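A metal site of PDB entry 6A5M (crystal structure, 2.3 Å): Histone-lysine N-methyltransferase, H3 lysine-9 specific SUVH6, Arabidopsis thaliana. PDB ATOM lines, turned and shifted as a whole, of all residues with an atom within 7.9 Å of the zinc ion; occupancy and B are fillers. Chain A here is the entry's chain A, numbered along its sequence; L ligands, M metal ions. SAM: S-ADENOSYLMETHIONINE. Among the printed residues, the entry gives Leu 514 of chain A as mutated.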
ATOM      1  N   HIS A 455       5.939 -18.277  18.546  1.00  0.00           N
ATOM      2  CA  HIS A 455       5.168 -18.373  19.778  1.00  0.00           C
ATOM      3  C   HIS A 455       3.684 -18.727  19.541  1.00  0.00           C
ATOM      4  O   HIS A 455       3.035 -18.186  18.647  1.00  0.00           O
ATOM      5  CB  HIS A 455       5.227 -17.059  20.556  1.00  0.00           C
ATOM      6  CG  HIS A 455       4.190 -16.971  21.622  1.00  0.00           C
ATOM      7  ND1 HIS A 455       4.377 -17.500  22.879  1.00  0.00           N
ATOM      8  CD2 HIS A 455       2.934 -16.467  21.606  1.00  0.00           C
ATOM      9  CE1 HIS A 455       3.278 -17.306  23.598  1.00  0.00           C
ATOM     10  NE2 HIS A 455       2.391 -16.691  22.848  1.00  0.00           N
ATOM     11  N   SER A 456       3.144 -19.600  20.370  1.00  0.00           N
ATOM     12  CA  SER A 456       1.699 -19.749  20.400  1.00  0.00           C
ATOM     13  C   SER A 456       1.198 -19.773  21.825  1.00  0.00           C
ATOM     14  O   SER A 456       1.871 -20.301  22.702  1.00  0.00           O
ATOM     15  CB  SER A 456       1.260 -21.019  19.679  1.00  0.00           C
ATOM     16  OG  SER A 456      -0.137 -21.185  19.839  1.00  0.00           O
ATOM     17  N   CYS A 457       0.023 -19.183  22.045  1.00  0.00           N
ATOM     18  CA  CYS A 457      -0.655 -19.260  23.337  1.00  0.00           C
ATOM     19  C   CYS A 457      -1.298 -20.629  23.548  1.00  0.00           C
ATOM     20  O   CYS A 457      -1.746 -20.959  24.638  1.00  0.00           O
ATOM     21  CB  CYS A 457      -1.733 -18.174  23.451  1.00  0.00           C
ATOM     22  SG  CYS A 457      -1.025 -16.526  23.465  1.00  0.00           S
ATOM     23  N   SER A 458      -1.330 -21.434  22.486  1.00  0.00           N
ATOM     24  CA  SER A 458      -1.781 -22.818  22.553  1.00  0.00           C
ATOM     25  C   SER A 458      -0.757 -23.717  21.850  1.00  0.00           C
ATOM     26  O   SER A 458      -1.021 -24.279  20.786  1.00  0.00           O
ATOM     27  CB  SER A 458      -3.158 -22.949  21.908  1.00  0.00           C
ATOM     28  OG  SER A 458      -3.718 -24.220  22.143  1.00  0.00           O
ATOM     29  N   LEU A 514       1.849  -7.218  19.831  1.00  0.00           N
ATOM     30  CA  LEU A 514       0.652  -8.054  19.751  1.00  0.00           C
ATOM     31  C   LEU A 514       0.981  -9.510  19.370  1.00  0.00           C
ATOM     32  O   LEU A 514       1.940  -9.757  18.635  1.00  0.00           O
ATOM     33  CB  LEU A 514      -0.339  -7.468  18.745  1.00  0.00           C
ATOM     34  CG  LEU A 514      -0.782  -6.048  19.107  1.00  0.00           C
ATOM     35  CD1 LEU A 514      -1.738  -5.450  18.075  1.00  0.00           C
ATOM     36  CD2 LEU A 514      -1.389  -6.048  20.495  1.00  0.00           C
ATOM     37  N   CYS A 515       0.200 -10.446  19.888  1.00  0.00           N
ATOM     38  CA  CYS A 515       0.358 -11.862  19.544  1.00  0.00           C
ATOM     39  C   CYS A 515      -0.621 -12.219  18.425  1.00  0.00           C
ATOM     40  O   CYS A 515      -1.813 -11.933  18.507  1.00  0.00           O
ATOM     41  CB  CYS A 515       0.108 -12.771  20.760  1.00  0.00           C
ATOM     42  SG  CYS A 515       0.244 -14.566  20.409  1.00  0.00           S
ATOM     43  N   PHE A 516      -0.086 -12.843  17.383  1.00  0.00           N
ATOM     44  CA  PHE A 516      -0.865 -13.208  16.224  1.00  0.00           C
ATOM     45  C   PHE A 516      -0.979 -14.731  16.125  1.00  0.00           C
ATOM     46  O   PHE A 516      -1.083 -15.259  15.027  1.00  0.00           O
ATOM     47  CB  PHE A 516      -0.234 -12.659  14.930  1.00  0.00           C
ATOM     48  CG  PHE A 516      -0.198 -11.147  14.823  1.00  0.00           C
ATOM     49  CD1 PHE A 516      -1.076 -10.348  15.548  1.00  0.00           C
ATOM     50  CD2 PHE A 516       0.718 -10.532  13.977  1.00  0.00           C
ATOM     51  CE1 PHE A 516      -1.037  -8.956  15.420  1.00  0.00           C
ATOM     52  CE2 PHE A 516       0.763  -9.133  13.845  1.00  0.00           C
ATOM     53  CZ  PHE A 516      -0.116  -8.344  14.581  1.00  0.00           C
ATOM     54  N   CYS A 517      -0.942 -15.433  17.246  1.00  0.00           N
ATOM     55  CA  CYS A 517      -0.882 -16.900  17.202  1.00  0.00           C
ATOM     56  C   CYS A 517      -2.198 -17.541  16.726  1.00  0.00           C
ATOM     57  O   CYS A 517      -2.207 -18.703  16.326  1.00  0.00           O
ATOM     58  CB  CYS A 517      -0.499 -17.463  18.577  1.00  0.00           C
ATOM     59  SG  CYS A 517      -1.858 -17.548  19.738  1.00  0.00           S
ATOM     60  N   GLY A 518      -3.296 -16.799  16.787  1.00  0.00           N
ATOM     61  CA  GLY A 518      -4.560 -17.253  16.251  1.00  0.00           C
ATOM     62  C   GLY A 518      -5.324 -18.231  17.122  1.00  0.00           C
ATOM     63  O   GLY A 518      -6.422 -18.657  16.762  1.00  0.00           O
ATOM     64  N   ALA A 519      -4.759 -18.602  18.273  1.00  0.00           N
ATOM     65  CA  ALA A 519      -5.410 -19.552  19.175  1.00  0.00           C
ATOM     66  C   ALA A 519      -6.694 -18.973  19.743  1.00  0.00           C
ATOM     67  O   ALA A 519      -6.798 -17.760  19.957  1.00  0.00           O
ATOM     68  CB  ALA A 519      -4.477 -19.963  20.307  1.00  0.00           C
ATOM     69  N   ALA A 520      -7.664 -19.842  19.998  1.00  0.00           N
ATOM     70  CA  ALA A 520      -8.962 -19.420  20.507  1.00  0.00           C
ATOM     71  C   ALA A 520      -8.829 -18.752  21.876  1.00  0.00           C
ATOM     72  O   ALA A 520      -9.588 -17.843  22.205  1.00  0.00           O
ATOM     73  CB  ALA A 520      -9.899 -20.619  20.587  1.00  0.00           C
ATOM     74  N   VAL A 521      -7.858 -19.190  22.657  1.00  0.00           N
ATOM     75  CA  VAL A 521      -7.576 -18.496  23.905  1.00  0.00           C
ATOM     76  C   VAL A 521      -6.172 -17.899  23.819  1.00  0.00           C
ATOM     77  O   VAL A 521      -5.198 -18.453  24.322  1.00  0.00           O
ATOM     78  CB  VAL A 521      -7.724 -19.430  25.120  1.00  0.00           C
ATOM     79  CG1 VAL A 521      -9.194 -19.648  25.436  1.00  0.00           C
ATOM     80  CG2 VAL A 521      -7.053 -20.745  24.861  1.00  0.00           C
ATOM     81  N   CYS A 522      -6.096 -16.768  23.140  1.00  0.00           N
ATOM     82  CA  CYS A 522      -4.856 -16.029  22.966  1.00  0.00           C
ATOM     83  C   CYS A 522      -4.760 -14.930  24.016  1.00  0.00           C
ATOM     84  O   CYS A 522      -5.738 -14.232  24.312  1.00  0.00           O
ATOM     85  CB  CYS A 522      -4.803 -15.435  21.548  1.00  0.00           C
ATOM     86  SG  CYS A 522      -3.469 -14.275  21.236  1.00  0.00           S
ATOM     87  N   ARG A 523      -3.573 -14.756  24.592  1.00  0.00           N
ATOM     88  CA  ARG A 523      -3.383 -13.750  25.616  1.00  0.00           C
ATOM     89  C   ARG A 523      -3.053 -12.387  24.985  1.00  0.00           C
ATOM     90  O   ARG A 523      -2.715 -11.437  25.689  1.00  0.00           O
ATOM     91  CB  ARG A 523      -2.285 -14.199  26.595  1.00  0.00           C
ATOM     92  CG  ARG A 523      -2.605 -15.562  27.217  1.00  0.00           C
ATOM     93  CD  ARG A 523      -1.657 -15.982  28.334  1.00  0.00           C
ATOM     94  NE  ARG A 523      -0.333 -16.322  27.826  1.00  0.00           N
ATOM     95  CZ  ARG A 523       0.000 -17.508  27.313  1.00  0.00           C
ATOM     96  NH1 ARG A 523      -0.894 -18.486  27.244  1.00  0.00           N
ATOM     97  NH2 ARG A 523       1.231 -17.712  26.883  1.00  0.00           N
ATOM     98  N   ARG A 524      -3.162 -12.320  23.667  1.00  0.00           N
ATOM     99  CA  ARG A 524      -3.260 -11.068  22.900  1.00  0.00           C
ATOM    100  C   ARG A 524      -1.989 -10.228  22.850  1.00  0.00           C
ATOM    101  O   ARG A 524      -1.798  -9.472  21.899  1.00  0.00           O
ATOM    102  CB  ARG A 524      -4.412 -10.214  23.459  1.00  0.00           C
ATOM    103  CG  ARG A 524      -5.770 -10.904  23.411  1.00  0.00           C
ATOM    104  CD  ARG A 524      -6.214 -11.308  21.992  1.00  0.00           C
ATOM    105  NE  ARG A 524      -6.159 -10.215  21.023  1.00  0.00           N
ATOM    106  CZ  ARG A 524      -7.103  -9.286  20.883  1.00  0.00           C
ATOM    107  NH1 ARG A 524      -8.176  -9.299  21.657  1.00  0.00           N
ATOM    108  NH2 ARG A 524      -6.966  -8.338  19.964  1.00  0.00           N
ATOM    109  N   ARG A 525      -1.125 -10.357  23.851  1.00  0.00           N
ATOM    110  CA  ARG A 525       0.153  -9.665  23.820  1.00  0.00           C
ATOM    111  C   ARG A 525       1.307 -10.655  23.978  1.00  0.00           C
ATOM    112  O   ARG A 525       1.245 -11.574  24.787  1.00  0.00           O
ATOM    113  CB  ARG A 525       0.231  -8.598  24.916  1.00  0.00           C
ATOM    114  CG  ARG A 525      -0.394  -7.273  24.531  1.00  0.00           C
ATOM    115  CD  ARG A 525      -0.254  -6.240  25.646  1.00  0.00           C
ATOM    116  NE  ARG A 525       1.156  -5.938  25.931  1.00  0.00           N
ATOM    117  CZ  ARG A 525       1.550  -5.137  26.923  1.00  0.00           C
ATOM    118  NH1 ARG A 525       0.659  -4.576  27.714  1.00  0.00           N
ATOM    119  NH2 ARG A 525       2.844  -4.919  27.124  1.00  0.00           N
ATOM    120  N   LEU A 526       2.341 -10.448  23.158  1.00  0.00           N
ATOM    121  CA  LEU A 526       3.565 -11.228  23.220  1.00  0.00           C
ATOM    122  C   LEU A 526       4.384 -10.745  24.418  1.00  0.00           C
ATOM    123  O   LEU A 526       4.957 -11.551  25.169  1.00  0.00           O
ATOM    124  CB  LEU A 526       4.336 -11.071  21.910  1.00  0.00           C
ATOM    125  CG  LEU A 526       5.292 -12.174  21.478  1.00  0.00           C
ATOM    126  CD1 LEU A 526       4.671 -13.536  21.713  1.00  0.00           C
ATOM    127  CD2 LEU A 526       5.647 -12.003  20.005  1.00  0.00           C
HETATM  128  N   SAM L   1       9.451 -15.313  13.136  1.00  0.00           N
HETATM  129  CA  SAM L   1      10.878 -15.204  13.379  1.00  0.00           C
HETATM  130  C   SAM L   1      11.630 -14.859  12.099  1.00  0.00           C
HETATM  131  O   SAM L   1      12.852 -14.762  12.098  1.00  0.00           O
HETATM  132  OXT SAM L   1      11.013 -14.666  11.052  1.00  0.00           O
HETATM  133  CB  SAM L   1      11.401 -16.490  13.999  1.00  0.00           C
HETATM  134  CG  SAM L   1      11.140 -16.530  15.495  1.00  0.00           C
HETATM  135  SD  SAM L   1      12.031 -15.184  16.360  1.00  0.00           S
HETATM  136  CE  SAM L   1      12.783 -16.168  17.690  1.00  0.00           C
HETATM  137  C5' SAM L   1      10.740 -14.317  17.285  1.00  0.00           C
HETATM  138  C4' SAM L   1       9.997 -13.225  16.504  1.00  0.00           C
HETATM  139  O4' SAM L   1       9.035 -13.787  15.610  1.00  0.00           O
HETATM  140  C3' SAM L   1       9.221 -12.295  17.421  1.00  0.00           C
HETATM  141  O3' SAM L   1       9.941 -11.135  17.773  1.00  0.00           O
HETATM  142  C2' SAM L   1       8.050 -11.871  16.565  1.00  0.00           C
HETATM  143  O2' SAM L   1       8.413 -10.774  15.764  1.00  0.00           O
HETATM  144  C1' SAM L   1       7.815 -13.075  15.674  1.00  0.00           C
HETATM  145  N9  SAM L   1       6.763 -13.893  16.325  1.00  0.00           N
HETATM  146  C8  SAM L   1       6.899 -15.172  16.848  1.00  0.00           C
HETATM  147  N7  SAM L   1       5.710 -15.563  17.346  1.00  0.00           N
HETATM  148  C5  SAM L   1       4.812 -14.553  17.188  1.00  0.00           C
HETATM  149  C6  SAM L   1       3.469 -14.406  17.537  1.00  0.00           C
HETATM  150  N6  SAM L   1       2.800 -15.381  18.151  1.00  0.00           N
HETATM  151  N1  SAM L   1       2.814 -13.243  17.214  1.00  0.00           N
HETATM  152  C2  SAM L   1       3.478 -12.214  16.579  1.00  0.00           C
HETATM  153  N3  SAM L   1       4.817 -12.362  16.246  1.00  0.00           N
HETATM  154  C4  SAM L   1       5.466 -13.506  16.539  1.00  0.00           C
HETATM  155 ZN    ZN M   1      -1.494 -15.706  21.224  1.00  0.00          ZN
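The backbone carbonyl oxygen of Arg 524 lies within hydrogen-bond range of the backbone NH of Cys 515.
The backbone NH (N) of Ala 519 sits close to the side-chain sulfur (SG) of Cys 517 (3.4 Å).
The backbone NH (N) of Arg 523 sits close to the side-chain sulfur (SG) of Cys 457 (3.3 Å).
The side-chain sulfur (SG) of Cys 457 lies close to a ring nitrogen (NE2) of His 455 (3.5 Å).
SG of Cys 522 sits close to N of Arg 524, 3.1 Å away.
The zinc ion is bound by the side-chain sulfur (SG) of Cys 515 (2.2 Å).
SG of Cys 517 is bound to the zinc ion.
The zinc ion is bound by the side-chain sulfur (SG) of Cys 457 (2.4 Å).
The zinc ion is bound by SG of Cys 522 (2.4 Å).
N6 of the ligand sits close to SG of Cys 515 (3.5 Å).
The backbone NH (N) of His 455 is in hydrogen-bond range of a nitrogen (N7) of the ligand (3.0 Å).
A nitrogen (N6) of the ligand is in hydrogen-bond range of the backbone carbonyl oxygen (O) of His 455 (2.9 Å).
N1 of the ligand sits at hydrogen-bond distance from N of Phe 516, at 2.9 Å.
Four residues have an atom within 4 Å of the zinc ion: Cys 457, Cys 515, Cys 517 and Cys 522.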
